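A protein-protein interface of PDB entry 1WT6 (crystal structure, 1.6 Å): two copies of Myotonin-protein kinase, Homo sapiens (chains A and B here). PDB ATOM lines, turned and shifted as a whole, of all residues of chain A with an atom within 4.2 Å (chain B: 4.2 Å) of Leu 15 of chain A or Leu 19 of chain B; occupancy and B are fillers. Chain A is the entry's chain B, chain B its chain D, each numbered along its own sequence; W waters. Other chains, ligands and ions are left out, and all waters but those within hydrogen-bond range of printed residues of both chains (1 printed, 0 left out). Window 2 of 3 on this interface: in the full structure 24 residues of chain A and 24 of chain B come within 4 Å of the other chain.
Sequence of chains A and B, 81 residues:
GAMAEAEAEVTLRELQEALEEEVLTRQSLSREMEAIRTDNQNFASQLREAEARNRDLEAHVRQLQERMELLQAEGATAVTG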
ATOM      1  N   THR A  11      23.127 -22.347 -32.404  1.00  0.00           N
ATOM      2  CA  THR A  11      23.848 -23.466 -31.855  1.00  0.00           C
ATOM      3  C   THR A  11      23.643 -23.470 -30.319  1.00  0.00           C
ATOM      4  O   THR A  11      23.329 -24.498 -29.756  1.00  0.00           O
ATOM      5  CB  THR A  11      25.325 -23.335 -32.165  1.00  0.00           C
ATOM      6  OG1 THR A  11      25.710 -22.005 -31.827  1.00  0.00           O
ATOM      7  CG2 THR A  11      25.569 -23.494 -33.613  1.00  0.00           C
ATOM      8  N   LEU A  12      23.790 -22.310 -29.667  1.00  0.00           N
ATOM      9  CA  LEU A  12      23.562 -22.202 -28.217  1.00  0.00           C
ATOM     10  C   LEU A  12      22.159 -22.727 -27.780  1.00  0.00           C
ATOM     11  O   LEU A  12      22.049 -23.549 -26.847  1.00  0.00           O
ATOM     12  CB  LEU A  12      23.834 -20.756 -27.721  1.00  0.00           C
ATOM     13  CG  LEU A  12      23.865 -20.615 -26.191  1.00  0.00           C
ATOM     14  CD1 LEU A  12      24.908 -21.552 -25.503  1.00  0.00           C
ATOM     15  CD2 LEU A  12      24.045 -19.168 -25.738  1.00  0.00           C
ATOM     16  N   ARG A  13      21.100 -22.300 -28.478  1.00  0.00           N
ATOM     17  CA  ARG A  13      19.736 -22.736 -28.136  1.00  0.00           C
ATOM     18  C   ARG A  13      19.522 -24.240 -28.402  1.00  0.00           C
ATOM     19  O   ARG A  13      18.837 -24.940 -27.621  1.00  0.00           O
ATOM     20  CB  ARG A  13      18.692 -21.891 -28.886  1.00  0.00           C
ATOM     21  CG  ARG A  13      17.226 -22.316 -28.693  1.00  0.00           C
ATOM     22  CD  ARG A  13      16.788 -22.493 -27.228  1.00  0.00           C
ATOM     23  NE  ARG A  13      15.395 -22.940 -27.172  1.00  0.00           N
ATOM     24  CZ  ARG A  13      14.837 -23.640 -26.169  1.00  0.00           C
ATOM     25  NH1 ARG A  13      15.543 -24.024 -25.096  1.00  0.00           N
ATOM     26  NH2 ARG A  13      13.556 -23.972 -26.250  1.00  0.00           N
ATOM     27  N   GLU A  14      20.111 -24.736 -29.487  1.00  0.00           N
ATOM     28  CA  GLU A  14      20.056 -26.176 -29.770  1.00  0.00           C
ATOM     29  C   GLU A  14      20.830 -26.974 -28.727  1.00  0.00           C
ATOM     30  O   GLU A  14      20.456 -28.088 -28.360  1.00  0.00           O
ATOM     31  CB  GLU A  14      20.545 -26.477 -31.183  1.00  0.00           C
ATOM     32  CG  GLU A  14      19.530 -25.954 -32.199  1.00  0.00           C
ATOM     33  CD  GLU A  14      19.927 -26.154 -33.652  1.00  0.00           C
ATOM     34  OE1 GLU A  14      21.078 -26.583 -33.920  1.00  0.00           O
ATOM     35  OE2 GLU A  14      19.069 -25.867 -34.530  1.00  0.00           O
ATOM     36  N   LEU A  15      21.901 -26.384 -28.225  1.00  0.00           N
ATOM     37  CA  LEU A  15      22.670 -27.022 -27.165  1.00  0.00           C
ATOM     38  C   LEU A  15      21.812 -27.113 -25.906  1.00  0.00           C
ATOM     39  O   LEU A  15      21.818 -28.141 -25.195  1.00  0.00           O
ATOM     40  CB  LEU A  15      23.906 -26.207 -26.865  1.00  0.00           C
ATOM     41  CG  LEU A  15      25.232 -26.931 -26.719  1.00  0.00           C
ATOM     42  CD1 LEU A  15      26.176 -26.161 -25.798  1.00  0.00           C
ATOM     43  CD2 LEU A  15      25.084 -28.395 -26.309  1.00  0.00           C
ATOM     44  N   GLN A  16      21.043 -26.063 -25.642  1.00  0.00           N
ATOM     45  CA  GLN A  16      20.199 -26.088 -24.438  1.00  0.00           C
ATOM     46  C   GLN A  16      19.156 -27.196 -24.567  1.00  0.00           C
ATOM     47  O   GLN A  16      18.861 -27.889 -23.588  1.00  0.00           O
ATOM     48  CB  GLN A  16      19.499 -24.757 -24.206  1.00  0.00           C
ATOM     49  CG  GLN A  16      18.569 -24.788 -22.975  1.00  0.00           C
ATOM     50  CD  GLN A  16      17.846 -23.468 -22.754  1.00  0.00           C
ATOM     51  OE1 GLN A  16      17.656 -23.045 -21.615  1.00  0.00           O
ATOM     52  NE2 GLN A  16      17.462 -22.797 -23.846  1.00  0.00           N
ATOM     53  N   GLU A  17      18.598 -27.334 -25.757  1.00  0.00           N
ATOM     54  CA  GLU A  17      17.563 -28.352 -26.000  1.00  0.00           C
ATOM     55  C   GLU A  17      18.169 -29.742 -25.882  1.00  0.00           C
ATOM     56  O   GLU A  17      17.544 -30.654 -25.313  1.00  0.00           O
ATOM     57  CB  GLU A  17      16.911 -28.123 -27.368  1.00  0.00           C
ATOM     58  CG  GLU A  17      16.061 -26.873 -27.377  1.00  0.00           C
ATOM     59  CD  GLU A  17      15.755 -26.386 -28.766  1.00  0.00           C
ATOM     60  OE1 GLU A  17      15.698 -27.225 -29.698  1.00  0.00           O
ATOM     61  OE2 GLU A  17      15.573 -25.155 -28.923  1.00  0.00           O
ATOM     62  N   ALA A  18      19.407 -29.903 -26.348  1.00  0.00           N
ATOM     63  CA  ALA A  18      20.029 -31.230 -26.268  1.00  0.00           C
ATOM     64  C   ALA A  18      20.261 -31.531 -24.794  1.00  0.00           C
ATOM     65  O   ALA A  18      20.127 -32.670 -24.357  1.00  0.00           O
ATOM     66  CB  ALA A  18      21.329 -31.302 -27.020  1.00  0.00           C
ATOM     67  N   LEU A  19      20.641 -30.515 -24.024  1.00  0.00           N
ATOM     68  CA  LEU A  19      20.926 -30.767 -22.610  1.00  0.00           C
ATOM     69  C   LEU A  19      19.643 -31.177 -21.887  1.00  0.00           C
ATOM     70  O   LEU A  19      19.629 -32.128 -21.108  1.00  0.00           O
ATOM     71  CB  LEU A  19      21.553 -29.545 -21.917  1.00  0.00           C
ATOM     72  CG  LEU A  19      21.708 -29.651 -20.383  1.00  0.00           C
ATOM     73  CD1 LEU A  19      22.586 -30.825 -19.947  1.00  0.00           C
ATOM     74  CD2 LEU A  19      22.198 -28.307 -19.807  1.00  0.00           C
ATOM     75  N   LEU B  15      31.490 -26.599 -24.852  1.00  0.00           N
ATOM     76  CA  LEU B  15      30.253 -27.046 -24.172  1.00  0.00           C
ATOM     77  C   LEU B  15      29.638 -28.228 -24.939  1.00  0.00           C
ATOM     78  O   LEU B  15      29.126 -29.171 -24.300  1.00  0.00           O
ATOM     79  CB  LEU B  15      29.262 -25.882 -24.038  1.00  0.00           C
ATOM     80  CG  LEU B  15      29.832 -24.808 -23.104  1.00  0.00           C
ATOM     81  CD1 LEU B  15      28.855 -23.597 -23.029  1.00  0.00           C
ATOM     82  CD2 LEU B  15      30.120 -25.404 -21.679  1.00  0.00           C
ATOM     83  N   GLN B  16      29.701 -28.190 -26.278  1.00  0.00           N
ATOM     84  CA  GLN B  16      29.063 -29.239 -27.141  1.00  0.00           C
ATOM     85  C   GLN B  16      29.805 -30.515 -26.864  1.00  0.00           C
ATOM     86  O   GLN B  16      29.209 -31.577 -26.606  1.00  0.00           O
ATOM     87  CB  GLN B  16      29.183 -28.858 -28.625  1.00  0.00           C
ATOM     88  CG  GLN B  16      28.102 -27.898 -29.050  1.00  0.00           C
ATOM     89  CD  GLN B  16      28.251 -27.356 -30.478  1.00  0.00           C
ATOM     90  OE1 GLN B  16      29.292 -26.796 -30.865  1.00  0.00           O
ATOM     91  NE2 GLN B  16      27.177 -27.463 -31.242  1.00  0.00           N
ATOM     92  N   GLU B  17      31.112 -30.404 -26.813  1.00  0.00           N
ATOM     93  CA  GLU B  17      31.961 -31.593 -26.539  1.00  0.00           C
ATOM     94  C   GLU B  17      31.760 -32.124 -25.121  1.00  0.00           C
ATOM     95  O   GLU B  17      31.763 -33.355 -24.895  1.00  0.00           O
ATOM     96  CB  GLU B  17      33.437 -31.260 -26.750  1.00  0.00           C
ATOM     97  CG  GLU B  17      33.737 -30.930 -28.191  1.00  0.00           C
ATOM     98  CD  GLU B  17      35.155 -30.466 -28.437  1.00  0.00           C
ATOM     99  OE1 GLU B  17      35.894 -30.180 -27.460  1.00  0.00           O
ATOM    100  OE2 GLU B  17      35.516 -30.391 -29.634  1.00  0.00           O
ATOM    101  N   ALA B  18      31.599 -31.206 -24.165  1.00  0.00           N
ATOM    102  CA  ALA B  18      31.410 -31.624 -22.790  1.00  0.00           C
ATOM    103  C   ALA B  18      30.034 -32.350 -22.678  1.00  0.00           C
ATOM    104  O   ALA B  18      29.878 -33.349 -21.919  1.00  0.00           O
ATOM    105  CB  ALA B  18      31.524 -30.432 -21.858  1.00  0.00           C
ATOM    106  N   LEU B  19      29.024 -31.871 -23.393  1.00  0.00           N
ATOM    107  CA  LEU B  19      27.743 -32.581 -23.349  1.00  0.00           C
ATOM    108  C   LEU B  19      27.874 -33.939 -24.006  1.00  0.00           C
ATOM    109  O   LEU B  19      27.409 -34.926 -23.456  1.00  0.00           O
ATOM    110  CB  LEU B  19      26.645 -31.795 -24.043  1.00  0.00           C
ATOM    111  CG  LEU B  19      25.301 -32.506 -24.082  1.00  0.00           C
ATOM    112  CD1 LEU B  19      24.783 -32.855 -22.695  1.00  0.00           C
ATOM    113  CD2 LEU B  19      24.336 -31.636 -24.886  1.00  0.00           C
ATOM    114  N   GLU B  20      28.561 -34.011 -25.158  1.00  0.00           N
ATOM    115  CA  GLU B  20      28.745 -35.337 -25.762  1.00  0.00           C
ATOM    116  C   GLU B  20      29.431 -36.327 -24.816  1.00  0.00           C
ATOM    117  O   GLU B  20      29.006 -37.504 -24.780  1.00  0.00           O
ATOM    118  CB  GLU B  20      29.486 -35.222 -27.080  1.00  0.00           C
ATOM    119  CG  GLU B  20      28.687 -34.583 -28.170  1.00  0.00           C
ATOM    120  CD  GLU B  20      29.572 -34.036 -29.355  1.00  0.00           C
ATOM    121  OE1 GLU B  20      30.814 -34.270 -29.398  1.00  0.00           O
ATOM    122  OE2 GLU B  20      29.020 -33.356 -30.252  1.00  0.00           O
ATOM    123  N   GLU B  21      30.453 -35.861 -24.059  1.00  0.00           N
ATOM    124  CA  GLU B  21      31.158 -36.751 -23.134  1.00  0.00           C
ATOM    125  C   GLU B  21      30.229 -37.216 -22.021  1.00  0.00           C
ATOM    126  O   GLU B  21      30.272 -38.407 -21.605  1.00  0.00           O
ATOM    127  CB  GLU B  21      32.454 -36.157 -22.566  1.00  0.00           C
ATOM    128  CG  GLU B  21      33.263 -37.249 -21.780  1.00  0.00           C
ATOM    129  CD  GLU B  21      33.350 -38.648 -22.488  1.00  0.00           C
ATOM    130  OE1 GLU B  21      34.043 -38.759 -23.541  1.00  0.00           O
ATOM    131  OE2 GLU B  21      32.757 -39.648 -21.970  1.00  0.00           O
ATOM    132  N   GLU B  22      29.412 -36.297 -21.512  1.00  0.00           N
ATOM    133  CA  GLU B  22      28.452 -36.640 -20.454  1.00  0.00           C
ATOM    134  C   GLU B  22      27.381 -37.646 -20.952  1.00  0.00           C
ATOM    135  O   GLU B  22      27.079 -38.631 -20.226  1.00  0.00           O
ATOM    136  CB  GLU B  22      27.821 -35.378 -19.857  1.00  0.00           C
ATOM    137  CG  GLU B  22      26.646 -35.686 -18.907  1.00  0.00           C
ATOM    138  CD  GLU B  22      27.032 -36.557 -17.720  1.00  0.00           C
ATOM    139  OE1 GLU B  22      28.236 -36.543 -17.321  1.00  0.00           O
ATOM    140  OE2 GLU B  22      26.118 -37.238 -17.182  1.00  0.00           O
ATOM    141  N   VAL B  23      26.851 -37.440 -22.171  1.00  0.00           N
ATOM    142  CA  VAL B  23      25.970 -38.407 -22.833  1.00  0.00           C
ATOM    143  C   VAL B  23      26.608 -39.801 -22.888  1.00  0.00           C
ATOM    144  O   VAL B  23      25.958 -40.819 -22.508  1.00  0.00           O
ATOM    145  CB  VAL B  23      25.478 -37.894 -24.204  1.00  0.00           C
ATOM    146  CG1 VAL B  23      24.767 -39.001 -24.924  1.00  0.00           C
ATOM    147  CG2 VAL B  23      24.507 -36.659 -24.019  1.00  0.00           C
HETATM  148  O   HOH W   1      24.309 -26.957 -30.868  1.00  0.00           O
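Among the printed residues, merely in contact across the chains: Leu 15 of chain A with Leu 15 of chain B (3.6 Å), Leu 15 of chain A with Leu 19 of chain B (3.6 Å), Ala 18 of chain A with Leu 19 of chain B (3.7 Å), Leu 15 of chain A with Gln 16 of chain B (3.8 Å) and Leu 19 of chain A with Leu 19 of chain B (3.96 Å).
Arg 13 of chain A touches none of the printed residues of chain B. Of the printed residues of chain B, Ala 18 of chain A touches Leu 19. Printed residues of chain B within 4 Å of Leu 19 of chain A: Leu 19. Printed residues of chain A within 4 Å of Leu 15 of chain B: Leu 15 (3.6 Å). Of the printed residues of chain A, Gln 16 of chain B touches Leu 15 (3.8 Å). Printed residues of chain A within 4 Å of Leu 19 of chain B: Leu 15 (3.6 Å), Ala 18 (3.7 Å) and Leu 19 (3.96 Å). The nearest printed residue of chain B that does not touch Leu 15 of chain A is Glu 17 of chain B (6.4 Å). The nearest printed residue of chain A that does not touch Leu 19 of chain B is Glu 14 of chain A (6.3 Å). The nearest printed residue of chain A that does not touch Gln 16 of chain B is Thr 11 of chain A (4.6 Å).
Of the 9 printed residues of chain B, 3 touch a printed residue of chain A. Hydrophobic or aromatic side chains of chain B that line the printed part of chain A: Leu 15 and Leu 19. Of the 9 printed residues of chain A, 3 touch a printed residue of chain B. Hydrophobic or aromatic side chains of chain A within 4 Å of the printed part of chain B: Leu 15 and Ala 18.
Leu 15 of chain A touches its own counterpart, Leu 15 of chain B. Leu 15 of chain A touches Gln 16 of chain B, but with the chains exchanged Gln 16 of chain A does not touch Leu 15 of chain B (8.4 Å). Leu 15 of chain A touches Leu 19 of chain B, but with the chains exchanged Leu 19 of chain A does not touch Leu 15 of chain B (7.9 Å). Leu 19 of chain B touches its own counterpart, Leu 19 of chain A. Positions printed for both chains: 15, 16, 17, 18 and 19. Of the 5 pairs that touch across the chains among the printed residues, 2 have their exchanged pair printed and touching as well.
Water W1 bridges O of Thr 11 of chain A (2.9 Å) and NE2 of Gln 16 of chain B (2.9 Å).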
